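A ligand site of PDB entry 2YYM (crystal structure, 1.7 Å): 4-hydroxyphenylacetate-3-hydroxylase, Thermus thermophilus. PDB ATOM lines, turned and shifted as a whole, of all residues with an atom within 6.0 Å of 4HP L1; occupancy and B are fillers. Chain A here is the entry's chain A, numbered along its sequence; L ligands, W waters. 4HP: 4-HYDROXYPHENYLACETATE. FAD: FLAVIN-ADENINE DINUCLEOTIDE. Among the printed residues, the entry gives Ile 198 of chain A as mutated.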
ATOM      1  N   ARG A 100      13.330 -21.436   2.653  1.00  0.00           N
ATOM      2  CA  ARG A 100      14.012 -20.917   3.825  1.00  0.00           C
ATOM      3  C   ARG A 100      13.115 -20.463   4.969  1.00  0.00           C
ATOM      4  O   ARG A 100      13.381 -19.440   5.596  1.00  0.00           O
ATOM      5  CB  ARG A 100      14.960 -19.768   3.438  1.00  0.00           C
ATOM      6  CG  ARG A 100      16.413 -20.198   3.260  1.00  0.00           C
ATOM      7  CD  ARG A 100      16.597 -21.074   2.035  1.00  0.00           C
ATOM      8  NE  ARG A 100      17.833 -21.851   2.114  1.00  0.00           N
ATOM      9  CZ  ARG A 100      18.002 -22.898   2.910  1.00  0.00           C
ATOM     10  NH1 ARG A 100      17.006 -23.310   3.690  1.00  0.00           N
ATOM     11  NH2 ARG A 100      19.171 -23.534   2.947  1.00  0.00           N
ATOM     12  N   TYR A 104      13.964 -24.175   9.671  1.00  0.00           N
ATOM     13  CA  TYR A 104      15.179 -24.827   9.181  1.00  0.00           C
ATOM     14  C   TYR A 104      16.354 -24.342  10.036  1.00  0.00           C
ATOM     15  O   TYR A 104      17.144 -25.133  10.531  1.00  0.00           O
ATOM     16  CB  TYR A 104      15.401 -24.453   7.706  1.00  0.00           C
ATOM     17  CG  TYR A 104      16.737 -24.856   7.090  1.00  0.00           C
ATOM     18  CD1 TYR A 104      16.964 -26.167   6.654  1.00  0.00           C
ATOM     19  CD2 TYR A 104      17.748 -23.911   6.898  1.00  0.00           C
ATOM     20  CE1 TYR A 104      18.163 -26.516   6.019  1.00  0.00           C
ATOM     21  CE2 TYR A 104      18.944 -24.250   6.264  1.00  0.00           C
ATOM     22  CZ  TYR A 104      19.145 -25.549   5.823  1.00  0.00           C
ATOM     23  OH  TYR A 104      20.313 -25.875   5.161  1.00  0.00           O
ATOM     24  N   LEU A 105      16.434 -23.027  10.214  1.00  0.00           N
ATOM     25  CA  LEU A 105      17.521 -22.451  11.010  1.00  0.00           C
ATOM     26  C   LEU A 105      17.302 -22.664  12.504  1.00  0.00           C
ATOM     27  O   LEU A 105      18.273 -22.739  13.265  1.00  0.00           O
ATOM     28  CB  LEU A 105      17.673 -20.959  10.684  1.00  0.00           C
ATOM     29  CG  LEU A 105      18.154 -20.669   9.259  1.00  0.00           C
ATOM     30  CD1 LEU A 105      18.257 -19.169   9.048  1.00  0.00           C
ATOM     31  CD2 LEU A 105      19.508 -21.329   9.026  1.00  0.00           C
ATOM     32  N   HIS A 142      20.050 -16.621   6.838  1.00  0.00           N
ATOM     33  CA  HIS A 142      21.472 -16.951   6.988  1.00  0.00           C
ATOM     34  C   HIS A 142      22.246 -16.850   5.683  1.00  0.00           C
ATOM     35  O   HIS A 142      21.668 -16.816   4.605  1.00  0.00           O
ATOM     36  CB  HIS A 142      21.632 -18.367   7.571  1.00  0.00           C
ATOM     37  CG  HIS A 142      21.339 -19.469   6.603  1.00  0.00           C
ATOM     38  ND1 HIS A 142      20.198 -19.504   5.827  1.00  0.00           N
ATOM     39  CD2 HIS A 142      22.025 -20.598   6.303  1.00  0.00           C
ATOM     40  CE1 HIS A 142      20.196 -20.602   5.092  1.00  0.00           C
ATOM     41  NE2 HIS A 142      21.296 -21.283   5.366  1.00  0.00           N
ATOM     42  N   LEU A 144      26.111 -18.467   4.387  1.00  0.00           N
ATOM     43  CA  LEU A 144      27.308 -19.236   4.724  1.00  0.00           C
ATOM     44  C   LEU A 144      28.415 -19.247   3.680  1.00  0.00           C
ATOM     45  O   LEU A 144      29.522 -19.710   3.967  1.00  0.00           O
ATOM     46  CB  LEU A 144      26.915 -20.700   5.004  1.00  0.00           C
ATOM     47  CG  LEU A 144      25.678 -21.011   5.841  1.00  0.00           C
ATOM     48  CD1 LEU A 144      25.570 -22.520   6.016  1.00  0.00           C
ATOM     49  CD2 LEU A 144      25.768 -20.321   7.203  1.00  0.00           C
ATOM     50  N   THR A 145      28.137 -18.740   2.480  1.00  0.00           N
ATOM     51  CA  THR A 145      29.125 -18.775   1.414  1.00  0.00           C
ATOM     52  C   THR A 145      29.832 -17.462   1.109  1.00  0.00           C
ATOM     53  O   THR A 145      29.290 -16.379   1.293  1.00  0.00           O
ATOM     54  CB  THR A 145      28.502 -19.308   0.106  1.00  0.00           C
ATOM     55  OG1 THR A 145      27.549 -18.364  -0.402  1.00  0.00           O
ATOM     56  CG2 THR A 145      27.792 -20.627   0.365  1.00  0.00           C
ATOM     57  N   PRO A 196      29.544 -20.786   9.696  1.00  0.00           N
ATOM     58  CA  PRO A 196      30.534 -21.407   8.809  1.00  0.00           C
ATOM     59  C   PRO A 196      29.884 -22.200   7.687  1.00  0.00           C
ATOM     60  O   PRO A 196      28.696 -22.516   7.731  1.00  0.00           O
ATOM     61  CB  PRO A 196      31.323 -22.316   9.748  1.00  0.00           C
ATOM     62  CG  PRO A 196      31.098 -21.734  11.113  1.00  0.00           C
ATOM     63  CD  PRO A 196      29.658 -21.336  11.061  1.00  0.00           C
ATOM     64  N   SER A 197      30.683 -22.525   6.673  1.00  0.00           N
ATOM     65  CA  SER A 197      30.180 -23.338   5.572  1.00  0.00           C
ATOM     66  C   SER A 197      30.014 -24.752   6.118  1.00  0.00           C
ATOM     67  O   SER A 197      30.787 -25.180   6.976  1.00  0.00           O
ATOM     68  CB  SER A 197      31.181 -23.347   4.419  1.00  0.00           C
ATOM     69  OG  SER A 197      30.855 -24.381   3.501  1.00  0.00           O
ATOM     70  N   ILE A 198      29.010 -25.449   5.619  1.00  0.00           N
ATOM     71  CA  ILE A 198      28.750 -26.815   6.072  1.00  0.00           C
ATOM     72  C   ILE A 198      29.721 -27.837   5.479  1.00  0.00           C
ATOM     73  O   ILE A 198      30.115 -28.778   6.156  1.00  0.00           O
ATOM     74  CB  ILE A 198      27.309 -27.264   5.735  1.00  0.00           C
ATOM     75  CG1 ILE A 198      26.305 -26.370   6.469  1.00  0.00           C
ATOM     76  CG2 ILE A 198      27.108 -28.718   6.120  1.00  0.00           C
ATOM     77  CD1 ILE A 198      24.869 -26.777   6.251  1.00  0.00           C
ATOM     78  N   LEU A 199      30.111 -27.637   4.218  1.00  0.00           N
ATOM     79  CA  LEU A 199      31.007 -28.598   3.584  1.00  0.00           C
ATOM     80  C   LEU A 199      32.376 -28.077   3.163  1.00  0.00           C
ATOM     81  O   LEU A 199      33.266 -28.872   2.848  1.00  0.00           O
ATOM     82  CB  LEU A 199      30.327 -29.217   2.356  1.00  0.00           C
ATOM     83  CG  LEU A 199      30.020 -28.300   1.172  1.00  0.00           C
ATOM     84  CD1 LEU A 199      29.680 -29.139  -0.057  1.00  0.00           C
ATOM     85  CD2 LEU A 199      28.878 -27.384   1.524  1.00  0.00           C
ATOM     86  N   LEU A 200      32.552 -26.755   3.157  1.00  0.00           N
ATOM     87  CA  LEU A 200      33.831 -26.176   2.765  1.00  0.00           C
ATOM     88  C   LEU A 200      34.693 -25.829   3.983  1.00  0.00           C
ATOM     89  O   LEU A 200      34.167 -25.587   5.073  1.00  0.00           O
ATOM     90  CB  LEU A 200      33.619 -24.924   1.920  1.00  0.00           C
ATOM     91  CG  LEU A 200      32.692 -25.059   0.702  1.00  0.00           C
ATOM     92  CD1 LEU A 200      32.653 -23.737  -0.039  1.00  0.00           C
ATOM     93  CD2 LEU A 200      33.204 -26.174  -0.221  1.00  0.00           C
ATOM     94  N   MET A 284      18.775 -30.040  10.520  1.00  0.00           N
ATOM     95  CA  MET A 284      18.397 -29.151   9.425  1.00  0.00           C
ATOM     96  C   MET A 284      18.022 -30.007   8.213  1.00  0.00           C
ATOM     97  O   MET A 284      17.123 -29.652   7.448  1.00  0.00           O
ATOM     98  CB  MET A 284      19.523 -28.165   9.107  1.00  0.00           C
ATOM     99  CG  MET A 284      20.774 -28.757   8.504  1.00  0.00           C
ATOM    100  SD  MET A 284      22.200 -27.679   8.798  1.00  0.00           S
ATOM    101  CE  MET A 284      21.800 -26.284   7.757  1.00  0.00           C
ATOM    102  N   PHE A 440      21.305 -26.579  -5.782  1.00  0.00           N
ATOM    103  CA  PHE A 440      22.411 -26.028  -4.986  1.00  0.00           C
ATOM    104  C   PHE A 440      22.249 -25.561  -3.533  1.00  0.00           C
ATOM    105  O   PHE A 440      23.256 -25.361  -2.855  1.00  0.00           O
ATOM    106  CB  PHE A 440      23.005 -24.837  -5.744  1.00  0.00           C
ATOM    107  CG  PHE A 440      23.827 -25.218  -6.937  1.00  0.00           C
ATOM    108  CD1 PHE A 440      25.070 -25.817  -6.780  1.00  0.00           C
ATOM    109  CD2 PHE A 440      23.382 -24.930  -8.233  1.00  0.00           C
ATOM    110  CE1 PHE A 440      25.868 -26.131  -7.889  1.00  0.00           C
ATOM    111  CE2 PHE A 440      24.164 -25.229  -9.343  1.00  0.00           C
ATOM    112  CZ  PHE A 440      25.408 -25.839  -9.178  1.00  0.00           C
ATOM    113  N   PHE A 441      21.030 -25.377  -3.041  1.00  0.00           N
ATOM    114  CA  PHE A 441      20.904 -24.828  -1.696  1.00  0.00           C
ATOM    115  C   PHE A 441      21.739 -25.478  -0.592  1.00  0.00           C
ATOM    116  O   PHE A 441      22.310 -24.780   0.244  1.00  0.00           O
ATOM    117  CB  PHE A 441      19.430 -24.740  -1.275  1.00  0.00           C
ATOM    118  CG  PHE A 441      18.890 -25.982  -0.632  1.00  0.00           C
ATOM    119  CD1 PHE A 441      19.073 -26.210   0.726  1.00  0.00           C
ATOM    120  CD2 PHE A 441      18.216 -26.926  -1.389  1.00  0.00           C
ATOM    121  CE1 PHE A 441      18.594 -27.378   1.321  1.00  0.00           C
ATOM    122  CE2 PHE A 441      17.734 -28.093  -0.817  1.00  0.00           C
ATOM    123  CZ  PHE A 441      17.926 -28.318   0.545  1.00  0.00           C
ATOM    124  N   PHE A 442      21.846 -26.813  -0.598  1.00  0.00           N
ATOM    125  CA  PHE A 442      22.606 -27.508   0.449  1.00  0.00           C
ATOM    126  C   PHE A 442      24.099 -27.591   0.144  1.00  0.00           C
ATOM    127  O   PHE A 442      24.880 -28.067   0.972  1.00  0.00           O
ATOM    128  CB  PHE A 442      22.035 -28.906   0.657  1.00  0.00           C
ATOM    129  CG  PHE A 442      21.757 -29.245   2.101  1.00  0.00           C
ATOM    130  CD1 PHE A 442      20.706 -30.104   2.431  1.00  0.00           C
ATOM    131  CD2 PHE A 442      22.524 -28.708   3.132  1.00  0.00           C
ATOM    132  CE1 PHE A 442      20.433 -30.428   3.762  1.00  0.00           C
ATOM    133  CE2 PHE A 442      22.260 -29.029   4.466  1.00  0.00           C
ATOM    134  CZ  PHE A 442      21.218 -29.892   4.776  1.00  0.00           C
ATOM    135  N   GLY A 443      24.499 -27.125  -1.037  1.00  0.00           N
ATOM    136  CA  GLY A 443      25.896 -27.161  -1.425  1.00  0.00           C
ATOM    137  C   GLY A 443      26.074 -27.636  -2.854  1.00  0.00           C
ATOM    138  O   GLY A 443      25.114 -28.069  -3.500  1.00  0.00           O
ATOM    139  N   ASP A 444      27.298 -27.533  -3.360  1.00  0.00           N
ATOM    140  CA  ASP A 444      27.633 -27.976  -4.699  1.00  0.00           C
ATOM    141  C   ASP A 444      27.650 -29.512  -4.697  1.00  0.00           C
ATOM    142  O   ASP A 444      28.428 -30.109  -3.953  1.00  0.00           O
ATOM    143  CB  ASP A 444      29.007 -27.413  -5.087  1.00  0.00           C
ATOM    144  CG  ASP A 444      29.580 -28.040  -6.343  1.00  0.00           C
ATOM    145  OD1 ASP A 444      28.824 -28.668  -7.124  1.00  0.00           O
ATOM    146  OD2 ASP A 444      30.807 -27.895  -6.557  1.00  0.00           O
HETATM  147  C8  4HP L   1      27.816 -24.149   2.291  1.00  0.00           C
HETATM  148  O1  4HP L   1      27.713 -24.041   3.492  1.00  0.00           O
HETATM  149  O2  4HP L   1      29.029 -24.175   1.729  1.00  0.00           O
HETATM  150  C7  4HP L   1      26.580 -24.231   1.398  1.00  0.00           C
HETATM  151  C1  4HP L   1      25.303 -24.108   2.201  1.00  0.00           C
HETATM  152  C2  4HP L   1      24.696 -25.259   2.760  1.00  0.00           C
HETATM  153  C3  4HP L   1      23.512 -25.125   3.520  1.00  0.00           C
HETATM  154  C4  4HP L   1      22.939 -23.851   3.719  1.00  0.00           C
HETATM  155  C5  4HP L   1      23.553 -22.707   3.150  1.00  0.00           C
HETATM  156  C6  4HP L   1      24.722 -22.837   2.397  1.00  0.00           C
HETATM  157  O4  4HP L   1      21.814 -23.723   4.452  1.00  0.00           O
HETATM  158  PA  FAD L   2      30.747 -22.209  -6.798  1.00  0.00           P
HETATM  159  O1A FAD L   2      31.645 -22.841  -5.810  1.00  0.00           O
HETATM  160  O2A FAD L   2      31.061 -20.836  -7.221  1.00  0.00           O
HETATM  161  O5B FAD L   2      30.752 -23.196  -8.074  1.00  0.00           O
HETATM  162  C5B FAD L   2      30.563 -22.724  -9.406  1.00  0.00           C
HETATM  163  C4B FAD L   2      31.046 -23.915 -10.248  1.00  0.00           C
HETATM  164  O4B FAD L   2      32.457 -24.176 -10.160  1.00  0.00           O
HETATM  165  C3B FAD L   2      30.367 -25.271 -10.118  1.00  0.00           C
HETATM  166  O3B FAD L   2      30.237 -26.004 -11.342  1.00  0.00           O
HETATM  167  C2B FAD L   2      31.327 -25.922  -9.127  1.00  0.00           C
HETATM  168  O2B FAD L   2      31.168 -27.344  -9.129  1.00  0.00           O
HETATM  169  C1B FAD L   2      32.711 -25.475  -9.604  1.00  0.00           C
HETATM  170  N9A FAD L   2      33.686 -25.449  -8.494  1.00  0.00           N
HETATM  171  C8A FAD L   2      33.996 -24.377  -7.766  1.00  0.00           C
HETATM  172  N7A FAD L   2      34.912 -24.648  -6.835  1.00  0.00           N
HETATM  173  C5A FAD L   2      35.159 -25.943  -6.969  1.00  0.00           C
HETATM  174  C6A FAD L   2      35.928 -26.950  -6.373  1.00  0.00           C
HETATM  175  N6A FAD L   2      36.777 -26.644  -5.396  1.00  0.00           N
HETATM  176  N1A FAD L   2      35.915 -28.213  -6.851  1.00  0.00           N
HETATM  177  C2A FAD L   2      35.221 -28.678  -7.873  1.00  0.00           C
HETATM  178  N3A FAD L   2      34.461 -27.749  -8.421  1.00  0.00           N
HETATM  179  C4A FAD L   2      34.409 -26.459  -8.032  1.00  0.00           C
HETATM  180  N1  FAD L   2      23.472 -19.875   0.798  1.00  0.00           N
HETATM  181  C2  FAD L   2      23.429 -19.340   2.091  1.00  0.00           C
HETATM  182  O2  FAD L   2      24.412 -19.492   2.804  1.00  0.00           O
HETATM  183  N3  FAD L   2      22.084 -19.066   2.393  1.00  0.00           N
HETATM  184  C4  FAD L   2      20.958 -19.208   1.562  1.00  0.00           C
HETATM  185  O4  FAD L   2      19.869 -18.894   2.040  1.00  0.00           O
HETATM  186  C4X FAD L   2      21.135 -19.723   0.285  1.00  0.00           C
HETATM  187  N5  FAD L   2      20.172 -19.722  -0.739  1.00  0.00           N
HETATM  188  C5X FAD L   2      20.306 -20.060  -2.095  1.00  0.00           C
HETATM  189  C6  FAD L   2      19.250 -19.884  -2.986  1.00  0.00           C
HETATM  190  C7  FAD L   2      19.477 -20.219  -4.322  1.00  0.00           C
HETATM  191  C7M FAD L   2      18.243 -19.976  -5.199  1.00  0.00           C
HETATM  192  C8  FAD L   2      20.706 -20.696  -4.776  1.00  0.00           C
HETATM  193  C8M FAD L   2      21.156 -21.095  -6.186  1.00  0.00           C
HETATM  194  C9  FAD L   2      21.728 -20.826  -3.840  1.00  0.00           C
HETATM  195  C9A FAD L   2      21.582 -20.526  -2.477  1.00  0.00           C
HETATM  196  N10 FAD L   2      22.526 -20.559  -1.434  1.00  0.00           N
HETATM  197  C10 FAD L   2      22.425 -20.085  -0.111  1.00  0.00           C
HETATM  198  C1' FAD L   2      23.939 -20.880  -1.748  1.00  0.00           C
HETATM  199  C2' FAD L   2      24.320 -22.322  -2.114  1.00  0.00           C
HETATM  200  O2' FAD L   2      24.490 -22.988  -0.868  1.00  0.00           O
HETATM  201  C3' FAD L   2      25.463 -22.443  -3.120  1.00  0.00           C
HETATM  202  O3' FAD L   2      24.991 -22.005  -4.399  1.00  0.00           O
HETATM  203  C4' FAD L   2      26.072 -23.846  -3.211  1.00  0.00           C
HETATM  204  O4' FAD L   2      26.691 -24.155  -1.962  1.00  0.00           O
HETATM  205  C5' FAD L   2      27.157 -23.884  -4.290  1.00  0.00           C
HETATM  206  O5' FAD L   2      28.210 -22.952  -4.041  1.00  0.00           O
HETATM  207  P   FAD L   2      28.494 -21.728  -5.049  1.00  0.00           P
HETATM  208  O1P FAD L   2      27.266 -21.188  -5.668  1.00  0.00           O
HETATM  209  O2P FAD L   2      29.424 -20.751  -4.419  1.00  0.00           O
HETATM  210  O3P FAD L   2      29.232 -22.420  -6.292  1.00  0.00           O
HETATM  211  O   HOH W   1      29.268 -23.691  -0.876  1.00  0.00           O
HETATM  212  O   HOH W   2      20.897 -22.668   1.302  1.00  0.00           O
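Residues that only touch 4HP L1: Leu 144, Thr 145, Leu 199, Leu 200, Phe 441 and Phe 442.
Hydrophobic or aromatic side chains within 4 Å of 4HP L1: Tyr 104, His 142, Leu 144, Ile 198, Leu 199, Leu 200 and Phe 442.
Of the 17 residues printed, 11 come within 4 Å of 4HP L1.
OG of Ser 197 is in hydrogen-bond range of N of Leu 199, at 3.4 Å.
The backbone NH (N) of Leu 200 is in hydrogen-bond range of the side-chain hydroxyl (OG) of Ser 197 (2.9 Å).
The guanidinium group of Arg 100 lies close to the side-chain hydroxyl of Tyr 104 (3.4 Å).
O2 of 4HP L1 lies within hydrogen-bond range of OG of Ser 197, 2.6 Å away.
O4 of 4HP L1 sits at hydrogen-bond distance from NE2 of His 142, at 2.7 Å.
OH of Tyr 104 lies within hydrogen-bond range of O4 of 4HP L1, 2.7 Å away.
An oxygen (O1) of 4HP L1 is in hydrogen-bond range of the backbone NH of Ile 198 (2.9 Å).
NH2 of Arg 100 lies within hydrogen-bond range of O4 of 4HP L1, at 3.0 Å.
The backbone carbonyl oxygen (O) of His 142 sits at hydrogen-bond distance from a nitrogen (N3) of FAD L2 (3.2 Å).
The backbone carbonyl oxygen of Phe 441 is in hydrogen-bond range of an oxygen (O2') of FAD L2, 3.0 Å away.
The backbone NH (N) of Leu 144 sits at hydrogen-bond distance from an oxygen (O2) of FAD L2 (2.5 Å).
The backbone carbonyl oxygen (O) of Phe 440 sits close to an oxygen (O2') of FAD L2 (3.3 Å).
O2B of FAD L2 is in hydrogen-bond range of OD2 of Asp 444 (2.7 Å).
Water W1 bridges an oxygen (O2) of 4HP L1 and an oxygen (O4') of FAD L2.
Water W2 lies within hydrogen-bond range of NH2 of Arg 100 (2.5 Å), O of Phe 441 (2.8 Å) and O4 of 4HP L1 (3.4 Å).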
